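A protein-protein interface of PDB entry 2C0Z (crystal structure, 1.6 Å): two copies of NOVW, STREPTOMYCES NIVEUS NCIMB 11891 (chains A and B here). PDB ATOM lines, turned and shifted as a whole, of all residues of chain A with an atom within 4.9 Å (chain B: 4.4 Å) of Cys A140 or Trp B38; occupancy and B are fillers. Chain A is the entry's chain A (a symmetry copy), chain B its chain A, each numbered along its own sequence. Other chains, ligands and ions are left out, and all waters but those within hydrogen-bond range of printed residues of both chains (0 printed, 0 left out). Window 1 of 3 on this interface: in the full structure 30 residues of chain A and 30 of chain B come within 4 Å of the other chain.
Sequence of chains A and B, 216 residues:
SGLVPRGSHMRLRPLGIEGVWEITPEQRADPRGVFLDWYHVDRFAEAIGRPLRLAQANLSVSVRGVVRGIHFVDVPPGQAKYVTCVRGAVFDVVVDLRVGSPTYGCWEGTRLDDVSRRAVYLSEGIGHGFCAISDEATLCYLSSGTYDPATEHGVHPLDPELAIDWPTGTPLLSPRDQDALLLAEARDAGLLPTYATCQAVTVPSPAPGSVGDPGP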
ATOM      1  N   TRP A  38       7.311  29.675 -15.368  1.00  0.00           N
ATOM      2  CA  TRP A  38       8.356  30.653 -15.063  1.00  0.00           C
ATOM      3  C   TRP A  38       9.337  30.956 -16.204  1.00  0.00           C
ATOM      4  O   TRP A  38      10.171  31.848 -16.061  1.00  0.00           O
ATOM      5  CB  TRP A  38       9.125  30.316 -13.775  1.00  0.00           C
ATOM      6  CG  TRP A  38       9.888  29.048 -13.731  1.00  0.00           C
ATOM      7  CD1 TRP A  38       9.388  27.792 -13.638  1.00  0.00           C
ATOM      8  CD2 TRP A  38      11.303  28.909 -13.724  1.00  0.00           C
ATOM      9  NE1 TRP A  38      10.407  26.877 -13.551  1.00  0.00           N
ATOM     10  CE2 TRP A  38      11.599  27.540 -13.616  1.00  0.00           C
ATOM     11  CE3 TRP A  38      12.365  29.811 -13.785  1.00  0.00           C
ATOM     12  CZ2 TRP A  38      12.919  27.053 -13.592  1.00  0.00           C
ATOM     13  CZ3 TRP A  38      13.656  29.324 -13.769  1.00  0.00           C
ATOM     14  CH2 TRP A  38      13.926  27.968 -13.653  1.00  0.00           C
ATOM     15  N   ALA A  57      21.596  23.373 -16.012  1.00  0.00           N
ATOM     16  CA  ALA A  57      20.629  23.771 -14.986  1.00  0.00           C
ATOM     17  C   ALA A  57      21.258  23.407 -13.662  1.00  0.00           C
ATOM     18  O   ALA A  57      21.818  22.314 -13.515  1.00  0.00           O
ATOM     19  CB  ALA A  57      19.286  23.076 -15.166  1.00  0.00           C
ATOM     20  N   ASN A  58      21.194  24.328 -12.705  1.00  0.00           N
ATOM     21  CA  ASN A  58      21.792  24.162 -11.389  1.00  0.00           C
ATOM     22  C   ASN A  58      20.799  24.491 -10.296  1.00  0.00           C
ATOM     23  O   ASN A  58      19.801  25.188 -10.528  1.00  0.00           O
ATOM     24  CB  ASN A  58      22.996  25.092 -11.210  1.00  0.00           C
ATOM     25  CG  ASN A  58      24.177  24.708 -12.106  1.00  0.00           C
ATOM     26  OD1 ASN A  58      24.351  25.262 -13.151  1.00  0.00           O
ATOM     27  ND2 ASN A  58      25.015  23.827 -11.631  1.00  0.00           N
ATOM     28  N   LEU A  59      21.083  23.956  -9.114  1.00  0.00           N
ATOM     29  CA  LEU A  59      20.379  24.299  -7.874  1.00  0.00           C
ATOM     30  C   LEU A  59      21.406  24.629  -6.820  1.00  0.00           C
ATOM     31  O   LEU A  59      22.472  24.036  -6.766  1.00  0.00           O
ATOM     32  CB  LEU A  59      19.451  23.181  -7.406  1.00  0.00           C
ATOM     33  CG  LEU A  59      18.212  22.977  -8.272  1.00  0.00           C
ATOM     34  CD1 LEU A  59      17.753  21.554  -8.246  1.00  0.00           C
ATOM     35  CD2 LEU A  59      17.106  23.862  -7.824  1.00  0.00           C
ATOM     36  N   TYR A  82      19.430  32.604 -16.008  1.00  0.00           N
ATOM     37  CA  TYR A  82      18.016  32.815 -15.722  1.00  0.00           C
ATOM     38  C   TYR A  82      17.773  32.172 -14.381  1.00  0.00           C
ATOM     39  O   TYR A  82      17.828  30.953 -14.249  1.00  0.00           O
ATOM     40  CB  TYR A  82      17.219  32.180 -16.863  1.00  0.00           C
ATOM     41  CG  TYR A  82      15.760  32.548 -16.996  1.00  0.00           C
ATOM     42  CD1 TYR A  82      14.810  31.911 -16.232  1.00  0.00           C
ATOM     43  CD2 TYR A  82      15.337  33.518 -17.894  1.00  0.00           C
ATOM     44  CE1 TYR A  82      13.458  32.220 -16.352  1.00  0.00           C
ATOM     45  CE2 TYR A  82      14.009  33.830 -18.035  1.00  0.00           C
ATOM     46  CZ  TYR A  82      13.055  33.165 -17.263  1.00  0.00           C
ATOM     47  OH  TYR A  82      11.732  33.468 -17.451  1.00  0.00           O
ATOM     48  N   VAL A  83      17.520  33.004 -13.380  1.00  0.00           N
ATOM     49  CA  VAL A  83      17.544  32.604 -11.982  1.00  0.00           C
ATOM     50  C   VAL A  83      16.210  32.806 -11.286  1.00  0.00           C
ATOM     51  O   VAL A  83      15.569  33.839 -11.451  1.00  0.00           O
ATOM     52  CB  VAL A  83      18.718  33.232 -11.200  1.00  0.00           C
ATOM     53  CG1 VAL A  83      18.592  34.730 -11.093  1.00  0.00           C
ATOM     54  CG2 VAL A  83      18.870  32.590  -9.821  1.00  0.00           C
ATOM     55  N   THR A  84      15.828  31.826 -10.451  1.00  0.00           N
ATOM     56  CA  THR A  84      14.645  31.959  -9.625  1.00  0.00           C
ATOM     57  C   THR A  84      14.822  31.285  -8.281  1.00  0.00           C
ATOM     58  O   THR A  84      15.684  30.421  -8.121  1.00  0.00           O
ATOM     59  CB  THR A  84      13.424  31.389 -10.385  1.00  0.00           C
ATOM     60  OG1 THR A  84      12.225  31.837  -9.778  1.00  0.00           O
ATOM     61  CG2 THR A  84      13.333  29.879 -10.335  1.00  0.00           C
ATOM     62  N   VAL A  86      13.154  28.871  -5.675  1.00  0.00           N
ATOM     63  CA  VAL A  86      12.086  27.850  -5.647  1.00  0.00           C
ATOM     64  C   VAL A  86      11.670  27.482  -4.224  1.00  0.00           C
ATOM     65  O   VAL A  86      10.654  26.812  -4.021  1.00  0.00           O
ATOM     66  CB  VAL A  86      12.438  26.607  -6.438  1.00  0.00           C
ATOM     67  CG1 VAL A  86      12.603  26.927  -7.940  1.00  0.00           C
ATOM     68  CG2 VAL A  86      13.656  25.919  -5.884  1.00  0.00           C
ATOM     69  N   THR A 138      16.644  28.046  -1.677  1.00  0.00           N
ATOM     70  CA  THR A 138      17.042  27.262  -2.827  1.00  0.00           C
ATOM     71  C   THR A 138      16.835  28.049  -4.118  1.00  0.00           C
ATOM     72  O   THR A 138      15.713  28.472  -4.415  1.00  0.00           O
ATOM     73  CB  THR A 138      16.165  25.988  -2.884  1.00  0.00           C
ATOM     74  OG1 THR A 138      16.275  25.259  -1.641  1.00  0.00           O
ATOM     75  CG2 THR A 138      16.652  25.046  -3.989  1.00  0.00           C
ATOM     76  N   LEU A 139      17.918  28.265  -4.856  1.00  0.00           N
ATOM     77  CA  LEU A 139      17.892  28.924  -6.149  1.00  0.00           C
ATOM     78  C   LEU A 139      18.014  27.878  -7.241  1.00  0.00           C
ATOM     79  O   LEU A 139      18.720  26.883  -7.079  1.00  0.00           O
ATOM     80  CB  LEU A 139      19.037  29.924  -6.285  1.00  0.00           C
ATOM     81  CG  LEU A 139      18.945  31.109  -5.371  1.00  0.00           C
ATOM     82  CD1 LEU A 139      20.092  32.037  -5.717  1.00  0.00           C
ATOM     83  CD2 LEU A 139      17.620  31.786  -5.535  1.00  0.00           C
ATOM     84  N   CYS A 140      17.289  28.092  -8.340  1.00  0.00           N
ATOM     85  CA  CYS A 140      17.404  27.301  -9.539  1.00  0.00           C
ATOM     86  C   CYS A 140      17.876  28.214 -10.661  1.00  0.00           C
ATOM     87  O   CYS A 140      17.362  29.339 -10.807  1.00  0.00           O
ATOM     88  CB  CYS A 140      16.054  26.679  -9.879  1.00  0.00           C
ATOM     89  SG  CYS A 140      16.086  25.592 -11.302  1.00  0.00           S
ATOM     90  N   TYR A 141      18.863  27.772 -11.426  1.00  0.00           N
ATOM     91  CA  TYR A 141      19.504  28.594 -12.442  1.00  0.00           C
ATOM     92  C   TYR A 141      19.481  27.824 -13.745  1.00  0.00           C
ATOM     93  O   TYR A 141      19.808  26.633 -13.760  1.00  0.00           O
ATOM     94  CB  TYR A 141      21.022  28.837 -12.135  1.00  0.00           C
ATOM     95  CG  TYR A 141      21.461  29.232 -10.755  1.00  0.00           C
ATOM     96  CD1 TYR A 141      21.411  28.327  -9.715  1.00  0.00           C
ATOM     97  CD2 TYR A 141      22.005  30.484 -10.514  1.00  0.00           C
ATOM     98  CE1 TYR A 141      21.867  28.651  -8.446  1.00  0.00           C
ATOM     99  CE2 TYR A 141      22.467  30.829  -9.243  1.00  0.00           C
ATOM    100  CZ  TYR A 141      22.387  29.907  -8.218  1.00  0.00           C
ATOM    101  OH  TYR A 141      22.826  30.214  -6.936  1.00  0.00           O
ATOM    102  N   LEU A 142      19.107  28.486 -14.825  1.00  0.00           N
ATOM    103  CA  LEU A 142      19.314  27.985 -16.176  1.00  0.00           C
ATOM    104  C   LEU A 142      20.386  28.848 -16.834  1.00  0.00           C
ATOM    105  O   LEU A 142      20.299  30.090 -16.790  1.00  0.00           O
ATOM    106  CB  LEU A 142      18.029  28.033 -16.973  1.00  0.00           C
ATOM    107  CG  LEU A 142      16.769  27.506 -16.274  1.00  0.00           C
ATOM    108  CD1 LEU A 142      15.553  27.658 -17.182  1.00  0.00           C
ATOM    109  CD2 LEU A 142      16.933  26.067 -15.863  1.00  0.00           C
ATOM    110  N   MET B  10      27.422  13.308 -12.034  1.00  0.00           N
ATOM    111  CA  MET B  10      26.200  13.090 -12.823  1.00  0.00           C
ATOM    112  C   MET B  10      26.221  11.728 -13.542  1.00  0.00           C
ATOM    113  O   MET B  10      27.259  11.253 -14.015  1.00  0.00           O
ATOM    114  CB  MET B  10      26.046  14.239 -13.814  1.00  0.00           C
ATOM    115  CG  MET B  10      24.821  14.109 -14.719  1.00  0.00           C
ATOM    116  SD  MET B  10      24.576  15.522 -15.771  1.00  0.00           S
ATOM    117  CE  MET B  10      23.882  16.631 -14.621  1.00  0.00           C
ATOM    118  N   ILE B  23      18.269  10.782 -14.259  1.00  0.00           N
ATOM    119  CA  ILE B  23      19.489  11.557 -14.111  1.00  0.00           C
ATOM    120  C   ILE B  23      19.820  11.738 -12.639  1.00  0.00           C
ATOM    121  O   ILE B  23      19.007  12.213 -11.855  1.00  0.00           O
ATOM    122  CB  ILE B  23      19.328  12.912 -14.803  1.00  0.00           C
ATOM    123  CG1 ILE B  23      18.999  12.719 -16.318  1.00  0.00           C
ATOM    124  CG2 ILE B  23      20.615  13.699 -14.652  1.00  0.00           C
ATOM    125  CD1 ILE B  23      17.504  12.723 -16.642  1.00  0.00           C
ATOM    126  N   PRO B  25      22.224  13.871 -10.280  1.00  0.00           N
ATOM    127  CA  PRO B  25      22.925  15.146 -10.449  1.00  0.00           C
ATOM    128  C   PRO B  25      24.405  15.048 -10.059  1.00  0.00           C
ATOM    129  O   PRO B  25      24.808  14.100  -9.383  1.00  0.00           O
ATOM    130  CB  PRO B  25      22.190  16.072  -9.482  1.00  0.00           C
ATOM    131  CG  PRO B  25      21.770  15.151  -8.374  1.00  0.00           C
ATOM    132  CD  PRO B  25      21.360  13.892  -9.090  1.00  0.00           C
ATOM    133  N   LEU B  36      24.390  21.773  -6.893  1.00  0.00           N
ATOM    134  CA  LEU B  36      24.305  20.707  -7.864  1.00  0.00           C
ATOM    135  C   LEU B  36      24.019  21.160  -9.274  1.00  0.00           C
ATOM    136  O   LEU B  36      23.378  22.173  -9.501  1.00  0.00           O
ATOM    137  CB  LEU B  36      23.271  19.677  -7.433  1.00  0.00           C
ATOM    138  CG  LEU B  36      21.853  20.158  -7.192  1.00  0.00           C
ATOM    139  CD1 LEU B  36      20.880  19.059  -7.579  1.00  0.00           C
ATOM    140  CD2 LEU B  36      21.651  20.619  -5.720  1.00  0.00           C
ATOM    141  N   ASP B  37      24.473  20.341 -10.207  1.00  0.00           N
ATOM    142  CA  ASP B  37      24.172  20.426 -11.644  1.00  0.00           C
ATOM    143  C   ASP B  37      23.118  19.349 -11.881  1.00  0.00           C
ATOM    144  O   ASP B  37      23.406  18.157 -11.707  1.00  0.00           O
ATOM    145  CB  ASP B  37      25.361  20.093 -12.572  1.00  0.00           C
ATOM    146  CG  ASP B  37      26.571  20.998 -12.396  1.00  0.00           C
ATOM    147  OD1 ASP B  37      26.442  22.130 -11.925  1.00  0.00           O
ATOM    148  OD2 ASP B  37      27.727  20.631 -12.733  1.00  0.00           O
ATOM    149  N   TRP B  38      21.908  19.736 -12.267  1.00  0.00           N
ATOM    150  CA  TRP B  38      20.859  18.757 -12.558  1.00  0.00           C
ATOM    151  C   TRP B  38      20.516  18.572 -14.042  1.00  0.00           C
ATOM    152  O   TRP B  38      19.727  17.688 -14.373  1.00  0.00           O
ATOM    153  CB  TRP B  38      19.580  19.000 -11.742  1.00  0.00           C
ATOM    154  CG  TRP B  38      18.855  20.275 -11.945  1.00  0.00           C
ATOM    155  CD1 TRP B  38      19.231  21.509 -11.528  1.00  0.00           C
ATOM    156  CD2 TRP B  38      17.592  20.442 -12.575  1.00  0.00           C
ATOM    157  NE1 TRP B  38      18.268  22.434 -11.841  1.00  0.00           N
ATOM    158  CE2 TRP B  38      17.251  21.803 -12.500  1.00  0.00           C
ATOM    159  CE3 TRP B  38      16.694  19.570 -13.191  1.00  0.00           C
ATOM    160  CZ2 TRP B  38      16.057  22.314 -13.042  1.00  0.00           C
ATOM    161  CZ3 TRP B  38      15.529  20.080 -13.727  1.00  0.00           C
ATOM    162  CH2 TRP B  38      15.208  21.427 -13.634  1.00  0.00           C
ATOM    163  N   TYR B  39      21.098  19.415 -14.908  1.00  0.00           N
ATOM    164  CA  TYR B  39      21.046  19.214 -16.366  1.00  0.00           C
ATOM    165  C   TYR B  39      22.357  19.715 -16.930  1.00  0.00           C
ATOM    166  O   TYR B  39      22.824  20.783 -16.555  1.00  0.00           O
ATOM    167  CB  TYR B  39      19.909  20.036 -17.025  1.00  0.00           C
ATOM    168  CG  TYR B  39      19.928  19.924 -18.540  1.00  0.00           C
ATOM    169  CD1 TYR B  39      19.377  18.813 -19.180  1.00  0.00           C
ATOM    170  CD2 TYR B  39      20.567  20.875 -19.321  1.00  0.00           C
ATOM    171  CE1 TYR B  39      19.441  18.683 -20.578  1.00  0.00           C
ATOM    172  CE2 TYR B  39      20.649  20.743 -20.677  1.00  0.00           C
ATOM    173  CZ  TYR B  39      20.081  19.635 -21.303  1.00  0.00           C
ATOM    174  OH  TYR B  39      20.157  19.507 -22.686  1.00  0.00           O
ATOM    175  N   TYR B  82      11.489  17.119 -18.628  1.00  0.00           N
ATOM    176  CA  TYR B  82      12.619  16.857 -17.745  1.00  0.00           C
ATOM    177  C   TYR B  82      12.208  17.379 -16.393  1.00  0.00           C
ATOM    178  O   TYR B  82      12.074  18.584 -16.198  1.00  0.00           O
ATOM    179  CB  TYR B  82      13.837  17.568 -18.336  1.00  0.00           C
ATOM    180  CG  TYR B  82      15.202  17.183 -17.817  1.00  0.00           C
ATOM    181  CD1 TYR B  82      15.684  17.734 -16.653  1.00  0.00           C
ATOM    182  CD2 TYR B  82      16.009  16.284 -18.501  1.00  0.00           C
ATOM    183  CE1 TYR B  82      16.947  17.409 -16.167  1.00  0.00           C
ATOM    184  CE2 TYR B  82      17.260  15.958 -18.044  1.00  0.00           C
ATOM    185  CZ  TYR B  82      17.741  16.536 -16.868  1.00  0.00           C
ATOM    186  OH  TYR B  82      19.009  16.223 -16.454  1.00  0.00           O
ATOM    187  N   THR B  84      12.131  17.354 -11.995  1.00  0.00           N
ATOM    188  CA  THR B  84      12.807  17.126 -10.734  1.00  0.00           C
ATOM    189  C   THR B  84      12.020  17.689  -9.568  1.00  0.00           C
ATOM    190  O   THR B  84      11.164  18.554  -9.748  1.00  0.00           O
ATOM    191  CB  THR B  84      14.229  17.734 -10.800  1.00  0.00           C
ATOM    192  OG1 THR B  84      15.026  17.212  -9.751  1.00  0.00           O
ATOM    193  CG2 THR B  84      14.255  19.232 -10.587  1.00  0.00           C
ATOM    194  N   CYS B 140       9.790  20.925 -10.481  1.00  0.00           N
ATOM    195  CA  CYS B 140      10.220  21.817 -11.529  1.00  0.00           C
ATOM    196  C   CYS B 140      10.333  21.011 -12.814  1.00  0.00           C
ATOM    197  O   CYS B 140      10.879  19.892 -12.803  1.00  0.00           O
ATOM    198  CB  CYS B 140      11.563  22.437 -11.159  1.00  0.00           C
ATOM    199  SG  CYS B 140      12.164  23.641 -12.342  1.00  0.00           S
ATOM    200  N   LEU B 142      11.150  21.116 -17.086  1.00  0.00           N
ATOM    201  CA  LEU B 142      11.575  21.733 -18.335  1.00  0.00           C
ATOM    202  C   LEU B 142      10.940  20.950 -19.480  1.00  0.00           C
ATOM    203  O   LEU B 142      11.023  19.708 -19.506  1.00  0.00           O
ATOM    204  CB  LEU B 142      13.083  21.726 -18.456  1.00  0.00           C
ATOM    205  CG  LEU B 142      13.872  22.166 -17.216  1.00  0.00           C
ATOM    206  CD1 LEU B 142      15.371  22.067 -17.476  1.00  0.00           C
ATOM    207  CD2 LEU B 142      13.508  23.569 -16.807  1.00  0.00           C
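Of the printed residues of chain B, Cys A140 touches Trp B38. Of chain A, only Ala A57 (2.9 Å), Asn A58 (3.4 Å), Leu A59 (3.6 Å) and Cys A140 (3.7 Å) come within 4 Å of Trp B38. Printed residues of chain B within 4 Å of Asn A58: Leu B36, Asp B37 and Trp B38. Printed residues of chain A within 4 Å of Asp B37: Ala A57 (3.6 Å) and Asn A58 (2.2 Å). Printed residues of chain A within 4 Å of Tyr B39: Ala A57 (2.9 Å). Val A83 touches none of the printed residues of chain B. The nearest printed residue of chain B that does not touch Asn A58 is Tyr B39 (5.4 Å).
The backbone NH (N) of Cys B140 is in hydrogen-bond range of the backbone carbonyl oxygen (O) of Thr B84 (2.8 Å). O of Trp B38 lies within hydrogen-bond range of OH of Tyr B82, 2.6 Å away. The side-chain hydroxyl (OH) of Tyr A82 sits at hydrogen-bond distance from the backbone carbonyl oxygen (O) of Trp A38, at 2.6 Å. The backbone carbonyl oxygen (O) of Thr A84 lies within hydrogen-bond range of the backbone NH (N) of Cys A140 (2.8 Å). The backbone NH (N) of Asn A58 lies within hydrogen-bond range of the backbone carbonyl oxygen (O) of Tyr A141.
The backbone NH (N) of Trp B38 lies within hydrogen-bond range of the backbone carbonyl oxygen (O) of Ala A57, at 2.9 Å. The indole nitrogen of Trp B38 lies within hydrogen-bond range of the backbone carbonyl oxygen of Asn A58. O of Leu B36 sits at hydrogen-bond distance from ND2 of Asn A58 (3.2 Å). The backbone NH (N) of Ala A57 lies within hydrogen-bond range of the backbone carbonyl oxygen (O) of Tyr B39 (2.9 Å). The backbone carbonyl oxygen of Leu B36 sits at hydrogen-bond distance from the backbone NH of Leu A59. OD1 of Asp B37 sits close to ND2 of Asn A58, at 2.2 Å.
Of the 13 printed residues of chain A, 5 touch a printed residue of chain B. Hydrophobic or aromatic side chains of chain A that line the printed part of chain B: Trp A38, Ala A57 and Leu A59. Printed residues of chain B that touch a printed residue of chain A: Leu B36, Asp B37, Trp B38, Tyr B39 and Cys B140. Along chain B the printed residues that touch a printed residue of chain A span positions 36 to 140. Among the printed residues, 10 pairs touch across the chains.
Trp A38 touches Cys B140. Asp B37 touches Ala A57. CD1 of Leu A59 touches CD1 of Trp B38, 3.6 Å away. Trp B38 touches Cys A140 (CZ2 to SG, 3.7 Å).
Trp A38 touches Cys B140, and with the chains exchanged Cys A140 touches Trp B38. Positions printed for both chains: 38, 82, 84, 140 and 142.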
